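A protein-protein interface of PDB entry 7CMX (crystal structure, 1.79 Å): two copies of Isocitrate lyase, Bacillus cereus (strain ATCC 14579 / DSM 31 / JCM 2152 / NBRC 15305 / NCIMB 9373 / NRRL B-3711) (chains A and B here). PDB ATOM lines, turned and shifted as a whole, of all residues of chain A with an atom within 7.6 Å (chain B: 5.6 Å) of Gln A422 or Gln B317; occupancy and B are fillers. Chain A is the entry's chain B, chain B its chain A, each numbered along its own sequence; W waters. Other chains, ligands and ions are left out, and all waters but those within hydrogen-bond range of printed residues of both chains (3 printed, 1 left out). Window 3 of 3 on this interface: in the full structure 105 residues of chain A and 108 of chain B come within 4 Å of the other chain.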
ATOM      1  N   SER A 369      13.881  -4.835   6.373  1.00  0.00           N
ATOM      2  CA  SER A 369      13.734  -4.992   7.841  1.00  0.00           C
ATOM      3  C   SER A 369      12.246  -5.081   8.241  1.00  0.00           C
ATOM      4  O   SER A 369      11.908  -5.921   9.086  1.00  0.00           O
ATOM      5  CB  SER A 369      14.432  -3.861   8.565  1.00  0.00           C
ATOM      6  OG  SER A 369      14.576  -4.179   9.934  1.00  0.00           O
ATOM      7  N   GLN A 372      11.227  -8.634   7.460  1.00  0.00           N
ATOM      8  CA  GLN A 372      11.902  -9.513   8.441  1.00  0.00           C
ATOM      9  C   GLN A 372      11.170  -9.468   9.799  1.00  0.00           C
ATOM     10  O   GLN A 372      11.011 -10.550  10.409  1.00  0.00           O
ATOM     11  CB  GLN A 372      13.375  -9.131   8.552  1.00  0.00           C
ATOM     12  CG  GLN A 372      14.171 -10.125   9.366  1.00  0.00           C
ATOM     13  CD  GLN A 372      15.626  -9.767   9.418  1.00  0.00           C
ATOM     14  OE1 GLN A 372      16.002  -8.712   9.925  1.00  0.00           O
ATOM     15  NE2 GLN A 372      16.455 -10.674   8.913  1.00  0.00           N
ATOM     16  N   GLN A 373      10.766  -8.290  10.280  1.00  0.00           N
ATOM     17  CA  GLN A 373      10.063  -8.173  11.585  1.00  0.00           C
ATOM     18  C   GLN A 373       8.643  -8.766  11.478  1.00  0.00           C
ATOM     19  O   GLN A 373       8.166  -9.379  12.436  1.00  0.00           O
ATOM     20  CB  GLN A 373      10.053  -6.709  12.027  1.00  0.00           C
ATOM     21  CG  GLN A 373      11.450  -6.187  12.324  1.00  0.00           C
ATOM     22  CD  GLN A 373      12.069  -6.893  13.499  1.00  0.00           C
ATOM     23  OE1 GLN A 373      11.398  -7.206  14.482  1.00  0.00           O
ATOM     24  NE2 GLN A 373      13.370  -7.135  13.432  1.00  0.00           N
ATOM     25  N   PHE A 376       9.138 -12.480  11.902  1.00  0.00           N
ATOM     26  CA  PHE A 376       9.341 -12.823  13.339  1.00  0.00           C
ATOM     27  C   PHE A 376       7.990 -12.874  14.054  1.00  0.00           C
ATOM     28  O   PHE A 376       7.763 -13.842  14.793  1.00  0.00           O
ATOM     29  CB  PHE A 376      10.241 -11.821  14.056  1.00  0.00           C
ATOM     30  CG  PHE A 376      11.701 -11.913  13.702  1.00  0.00           C
ATOM     31  CD1 PHE A 376      12.355 -13.136  13.666  1.00  0.00           C
ATOM     32  CD2 PHE A 376      12.434 -10.765  13.459  1.00  0.00           C
ATOM     33  CE1 PHE A 376      13.717 -13.190  13.398  1.00  0.00           C
ATOM     34  CE2 PHE A 376      13.787 -10.827  13.168  1.00  0.00           C
ATOM     35  CZ  PHE A 376      14.419 -12.039  13.122  1.00  0.00           C
ATOM     36  N   SER A 417      27.108 -20.315  12.330  1.00  0.00           N
ATOM     37  CA  SER A 417      26.236 -19.573  11.386  1.00  0.00           C
ATOM     38  C   SER A 417      25.708 -18.288  12.031  1.00  0.00           C
ATOM     39  O   SER A 417      25.512 -18.245  13.265  1.00  0.00           O
ATOM     40  CB  SER A 417      25.082 -20.418  10.915  1.00  0.00           C
ATOM     41  OG  SER A 417      24.212 -20.735  11.984  1.00  0.00           O
ATOM     42  N   THR A 418      25.381 -17.296  11.212  1.00  0.00           N
ATOM     43  CA  THR A 418      24.745 -16.058  11.711  1.00  0.00           C
ATOM     44  C   THR A 418      23.351 -16.428  12.210  1.00  0.00           C
ATOM     45  O   THR A 418      22.884 -15.750  13.117  1.00  0.00           O
ATOM     46  CB  THR A 418      24.713 -14.951  10.662  1.00  0.00           C
ATOM     47  OG1 THR A 418      23.934 -15.475   9.586  1.00  0.00           O
ATOM     48  CG2 THR A 418      26.099 -14.520  10.221  1.00  0.00           C
ATOM     49  N   GLU A 419      22.762 -17.525  11.719  1.00  0.00           N
ATOM     50  CA  GLU A 419      21.412 -17.976  12.163  1.00  0.00           C
ATOM     51  C   GLU A 419      21.479 -18.375  13.645  1.00  0.00           C
ATOM     52  O   GLU A 419      20.604 -17.951  14.405  1.00  0.00           O
ATOM     53  CB  GLU A 419      20.883 -19.114  11.272  1.00  0.00           C
ATOM     54  CG  GLU A 419      19.523 -19.639  11.689  1.00  0.00           C
ATOM     55  CD  GLU A 419      18.735 -20.348  10.583  1.00  0.00           C
ATOM     56  OE1 GLU A 419      18.421 -19.668   9.559  1.00  0.00           O
ATOM     57  OE2 GLU A 419      18.455 -21.591  10.725  1.00  0.00           O
ATOM     58  N   GLU A 420      22.481 -19.155  14.051  1.00  0.00           N
ATOM     59  CA  GLU A 420      22.632 -19.577  15.472  1.00  0.00           C
ATOM     60  C   GLU A 420      23.032 -18.367  16.336  1.00  0.00           C
ATOM     61  O   GLU A 420      22.598 -18.325  17.489  1.00  0.00           O
ATOM     62  CB  GLU A 420      23.607 -20.749  15.624  1.00  0.00           C
ATOM     63  CG  GLU A 420      22.940 -22.107  15.391  1.00  0.00           C
ATOM     64  CD  GLU A 420      23.714 -23.326  15.880  1.00  0.00           C
ATOM     65  OE1 GLU A 420      24.825 -23.147  16.464  1.00  0.00           O
ATOM     66  OE2 GLU A 420      23.219 -24.456  15.661  1.00  0.00           O
ATOM     67  N   ALA A 421      23.793 -17.413  15.802  1.00  0.00           N
ATOM     68  CA  ALA A 421      24.331 -16.250  16.555  1.00  0.00           C
ATOM     69  C   ALA A 421      23.272 -15.152  16.724  1.00  0.00           C
ATOM     70  O   ALA A 421      23.240 -14.531  17.811  1.00  0.00           O
ATOM     71  CB  ALA A 421      25.535 -15.709  15.855  1.00  0.00           C
ATOM     72  N   GLN A 422      22.418 -14.936  15.719  1.00  0.00           N
ATOM     73  CA  GLN A 422      21.613 -13.686  15.588  1.00  0.00           C
ATOM     74  C   GLN A 422      20.117 -13.960  15.716  1.00  0.00           C
ATOM     75  O   GLN A 422      19.374 -12.984  15.859  1.00  0.00           O
ATOM     76  CB  GLN A 422      21.930 -12.993  14.259  1.00  0.00           C
ATOM     77  CG  GLN A 422      23.334 -12.424  14.242  1.00  0.00           C
ATOM     78  CD  GLN A 422      23.642 -11.573  13.043  1.00  0.00           C
ATOM     79  OE1 GLN A 422      22.763 -10.890  12.511  1.00  0.00           O
ATOM     80  NE2 GLN A 422      24.898 -11.611  12.618  1.00  0.00           N
ATOM     81  N   PHE A 423      19.693 -15.225  15.692  1.00  0.00           N
ATOM     82  CA  PHE A 423      18.257 -15.585  15.714  1.00  0.00           C
ATOM     83  C   PHE A 423      18.016 -16.396  16.997  1.00  0.00           C
ATOM     84  O   PHE A 423      16.943 -16.992  17.003  1.00  0.00           O
ATOM     85  CB  PHE A 423      17.885 -16.234  14.374  1.00  0.00           C
ATOM     86  CG  PHE A 423      17.983 -15.324  13.161  1.00  0.00           C
ATOM     87  CD1 PHE A 423      19.218 -14.979  12.615  1.00  0.00           C
ATOM     88  CD2 PHE A 423      16.840 -14.819  12.555  1.00  0.00           C
ATOM     89  CE1 PHE A 423      19.303 -14.142  11.514  1.00  0.00           C
ATOM     90  CE2 PHE A 423      16.926 -13.989  11.443  1.00  0.00           C
ATOM     91  CZ  PHE A 423      18.158 -13.659  10.916  1.00  0.00           C
ATOM     92  N   SER B 282      29.972 -10.762   8.659  1.00  0.00           N
ATOM     93  CA  SER B 282      29.099 -11.466   9.624  1.00  0.00           C
ATOM     94  C   SER B 282      28.017 -10.500  10.123  1.00  0.00           C
ATOM     95  O   SER B 282      27.117 -10.960  10.819  1.00  0.00           O
ATOM     96  CB  SER B 282      29.915 -12.032  10.732  1.00  0.00           C
ATOM     97  OG  SER B 282      30.684 -10.979  11.300  1.00  0.00           O
ATOM     98  N   GLU B 283      28.095  -9.205   9.786  1.00  0.00           N
ATOM     99  CA  GLU B 283      27.036  -8.224  10.148  1.00  0.00           C
ATOM    100  C   GLU B 283      27.145  -6.956   9.304  1.00  0.00           C
ATOM    101  O   GLU B 283      28.177  -6.671   8.707  1.00  0.00           O
ATOM    102  CB  GLU B 283      27.137  -7.871  11.633  1.00  0.00           C
ATOM    103  CG  GLU B 283      28.423  -7.175  12.009  1.00  0.00           C
ATOM    104  CD  GLU B 283      28.453  -6.830  13.484  1.00  0.00           C
ATOM    105  OE1 GLU B 283      28.869  -5.711  13.805  1.00  0.00           O
ATOM    106  OE2 GLU B 283      28.000  -7.670  14.295  1.00  0.00           O
ATOM    107  N   SER B 312      20.383 -12.900   6.142  1.00  0.00           N
ATOM    108  CA  SER B 312      21.033 -13.755   7.170  1.00  0.00           C
ATOM    109  C   SER B 312      21.408 -12.925   8.401  1.00  0.00           C
ATOM    110  O   SER B 312      21.689 -13.510   9.458  1.00  0.00           O
ATOM    111  CB  SER B 312      22.205 -14.506   6.600  1.00  0.00           C
ATOM    112  OG  SER B 312      21.747 -15.508   5.713  1.00  0.00           O
ATOM    113  N   PHE B 313      21.416 -11.608   8.271  1.00  0.00           N
ATOM    114  CA  PHE B 313      21.576 -10.659   9.401  1.00  0.00           C
ATOM    115  C   PHE B 313      20.202 -10.378  10.013  1.00  0.00           C
ATOM    116  O   PHE B 313      19.177 -10.335   9.301  1.00  0.00           O
ATOM    117  CB  PHE B 313      22.185  -9.325   8.966  1.00  0.00           C
ATOM    118  CG  PHE B 313      23.500  -9.412   8.234  1.00  0.00           C
ATOM    119  CD1 PHE B 313      24.348 -10.488   8.408  1.00  0.00           C
ATOM    120  CD2 PHE B 313      23.878  -8.415   7.354  1.00  0.00           C
ATOM    121  CE1 PHE B 313      25.556 -10.551   7.731  1.00  0.00           C
ATOM    122  CE2 PHE B 313      25.085  -8.478   6.671  1.00  0.00           C
ATOM    123  CZ  PHE B 313      25.922  -9.547   6.858  1.00  0.00           C
ATOM    124  N   ASN B 314      20.190 -10.229  11.329  1.00  0.00           N
ATOM    125  CA  ASN B 314      19.044  -9.700  12.087  1.00  0.00           C
ATOM    126  C   ASN B 314      19.224  -8.186  12.110  1.00  0.00           C
ATOM    127  O   ASN B 314      19.936  -7.710  12.991  1.00  0.00           O
ATOM    128  CB  ASN B 314      19.009 -10.290  13.487  1.00  0.00           C
ATOM    129  CG  ASN B 314      17.773  -9.885  14.238  1.00  0.00           C
ATOM    130  OD1 ASN B 314      17.170  -8.859  13.953  1.00  0.00           O
ATOM    131  ND2 ASN B 314      17.380 -10.719  15.171  1.00  0.00           N
ATOM    132  N   TRP B 315      18.653  -7.478  11.134  1.00  0.00           N
ATOM    133  CA  TRP B 315      18.954  -6.034  10.913  1.00  0.00           C
ATOM    134  C   TRP B 315      18.636  -5.189  12.153  1.00  0.00           C
ATOM    135  O   TRP B 315      19.510  -4.410  12.578  1.00  0.00           O
ATOM    136  CB  TRP B 315      18.262  -5.540   9.653  1.00  0.00           C
ATOM    137  CG  TRP B 315      19.023  -5.992   8.446  1.00  0.00           C
ATOM    138  CD1 TRP B 315      18.978  -7.227   7.871  1.00  0.00           C
ATOM    139  CD2 TRP B 315      20.024  -5.254   7.734  1.00  0.00           C
ATOM    140  NE1 TRP B 315      19.847  -7.289   6.819  1.00  0.00           N
ATOM    141  CE2 TRP B 315      20.500  -6.096   6.710  1.00  0.00           C
ATOM    142  CE3 TRP B 315      20.531  -3.954   7.829  1.00  0.00           C
ATOM    143  CZ2 TRP B 315      21.461  -5.680   5.800  1.00  0.00           C
ATOM    144  CZ3 TRP B 315      21.499  -3.548   6.939  1.00  0.00           C
ATOM    145  CH2 TRP B 315      21.936  -4.397   5.923  1.00  0.00           C
ATOM    146  N   LYS B 316      17.456  -5.354  12.738  1.00  0.00           N
ATOM    147  CA  LYS B 316      17.025  -4.580  13.926  1.00  0.00           C
ATOM    148  C   LYS B 316      17.937  -4.906  15.115  1.00  0.00           C
ATOM    149  O   LYS B 316      18.163  -4.019  15.918  1.00  0.00           O
ATOM    150  CB  LYS B 316      15.546  -4.849  14.212  1.00  0.00           C
ATOM    151  CG  LYS B 316      14.711  -3.625  14.593  1.00  0.00           C
ATOM    152  CD  LYS B 316      13.366  -3.955  15.224  1.00  0.00           C
ATOM    153  CE  LYS B 316      13.518  -4.659  16.560  1.00  0.00           C
ATOM    154  NZ  LYS B 316      12.227  -4.893  17.255  1.00  0.00           N
ATOM    155  N   GLN B 317      18.468  -6.125  15.241  1.00  0.00           N
ATOM    156  CA  GLN B 317      19.402  -6.456  16.358  1.00  0.00           C
ATOM    157  C   GLN B 317      20.722  -5.705  16.156  1.00  0.00           C
ATOM    158  O   GLN B 317      21.400  -5.394  17.154  1.00  0.00           O
ATOM    159  CB  GLN B 317      19.636  -7.963  16.476  1.00  0.00           C
ATOM    160  CG  GLN B 317      20.534  -8.368  17.636  1.00  0.00           C
ATOM    161  CD  GLN B 317      20.889  -9.836  17.571  1.00  0.00           C
ATOM    162  OE1 GLN B 317      20.113 -10.712  17.963  1.00  0.00           O
ATOM    163  NE2 GLN B 317      22.058 -10.115  17.023  1.00  0.00           N
ATOM    164  N   LYS B 318      21.099  -5.416  14.913  1.00  0.00           N
ATOM    165  CA  LYS B 318      22.456  -4.879  14.624  1.00  0.00           C
ATOM    166  C   LYS B 318      22.461  -3.360  14.500  1.00  0.00           C
ATOM    167  O   LYS B 318      23.511  -2.796  14.779  1.00  0.00           O
ATOM    168  CB  LYS B 318      23.004  -5.525  13.352  1.00  0.00           C
ATOM    169  CG  LYS B 318      23.271  -7.016  13.502  1.00  0.00           C
ATOM    170  CD  LYS B 318      24.144  -7.340  14.691  1.00  0.00           C
ATOM    171  CE  LYS B 318      24.409  -8.818  14.847  1.00  0.00           C
ATOM    172  NZ  LYS B 318      25.410  -9.069  15.907  1.00  0.00           N
ATOM    173  N   LEU B 319      21.372  -2.753  14.024  1.00  0.00           N
ATOM    174  CA  LEU B 319      21.340  -1.324  13.623  1.00  0.00           C
ATOM    175  C   LEU B 319      20.035  -0.703  14.100  1.00  0.00           C
ATOM    176  O   LEU B 319      18.975  -1.401  14.070  1.00  0.00           O
ATOM    177  CB  LEU B 319      21.452  -1.197  12.102  1.00  0.00           C
ATOM    178  CG  LEU B 319      22.737  -1.713  11.456  1.00  0.00           C
ATOM    179  CD1 LEU B 319      22.661  -1.561   9.938  1.00  0.00           C
ATOM    180  CD2 LEU B 319      23.965  -0.986  11.998  1.00  0.00           C
HETATM  181  O   HOH W   1      20.846 -16.254   9.246  1.00  0.00           O
HETATM  182  O   HOH W   2      15.092  -6.470  11.245  1.00  0.00           O
HETATM  183  O   HOH W   3      15.005  -8.151  15.626  1.00  0.00           O
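The side-chain amide oxygen of Asn B314 sits at hydrogen-bond distance from the backbone NH of Gln B317.
NZ of Lys B318 is in salt-bridge range of OE2 of Glu B283.
Water W2 lies within hydrogen-bond range of OG of Ser A369 (2.7 Å), OE1 of Gln A372 (2.8 Å), NE2 of Gln A373 (2.9 Å) and N of Lys B316 (3.0 Å).
Water W3 bridges the side-chain amide oxygen (OD1) of Asn B314 (2.8 Å) and the side-chain amide nitrogen (NE2) of Gln A373 (2.9 Å).
Water W1 lies within hydrogen-bond range of the backbone carbonyl oxygen of Ser B312, the side-chain hydroxyl of Thr A418 and the backbone NH of Glu A419.
Trp B315 touches Ser A369 (CB to OG, 3.9 Å).
CA of Asn B314 touches OE1 of Gln A372, 3.9 Å away.
Gln A373 touches Lys B316.
Phe A376 touches Asn B314.
Thr A418 touches Ser B282.
CA of Phe B313 touches OE1 of Gln A422 (3.3 Å).
CD of Gln A422 touches CE of Lys B318 (3.4 Å).
O of Ser B312 touches CE1 of Phe A423 (3.2 Å).
Phe A423 touches Phe B313.
No position is printed for both chains.
Of the 15 pairs that touch across the chains among the printed residues, none has its exchanged pair printed and touching as well.
The backbone NH (N) of Asn B314 sits at hydrogen-bond distance from the side-chain amide oxygen (OE1) of Gln A422 (2.9 Å).
The backbone carbonyl oxygen (O) of Ser B312 is in hydrogen-bond range of the side-chain hydroxyl (OG1) of Thr A418 (3.0 Å).
OE1 of Gln B317 lies close to O of Gln A422, at 3.2 Å.
O of Phe B313 is in hydrogen-bond range of NE2 of Gln A372 (2.8 Å).
The side-chain amide nitrogen of Gln A422 is in hydrogen-bond range of the backbone carbonyl oxygen of Ser B282 (2.9 Å).
The backbone NH of Trp B315 is in hydrogen-bond range of the side-chain amide oxygen of Gln A372.
Of the printed residues of chain B, Gln A372 touches Phe B313 (2.8 Å), Asn B314 (3.9 Å) and Trp B315 (3.2 Å).
Of chain B, only Ser B282 (2.9 Å), Phe B313 (3.3 Å), Asn B314 (2.9 Å), Gln B317 (3.2 Å) and Lys B318 (3.4 Å) come within 4 Å of Gln A422.
Of the printed residues of chain B, Phe A423 touches Ser B312 (3.2 Å) and Phe B313 (3.8 Å).
Printed residues of chain A within 4 Å of Lys B316: Gln A373.
Of the printed residues of chain A, Gln B317 touches Gln A422 (3.2 Å).
The nearest residue of chain A that does not touch Gln B317 is Ala A421 (4.6 Å).
Hydrophobic or aromatic side chains of chain B that line the printed part of chain A: Phe B313 and Trp B315.
Printed residues of chain A that touch a printed residue of chain B: Ser A369, Gln A372, Gln A373, Phe A376, Thr A418, Gln A422 and Phe A423.
Hydrophobic or aromatic side chains of chain A that line the printed part of chain B: Phe A376 and Phe A423.
Among the printed residues, 15 pairs touch across the chains.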
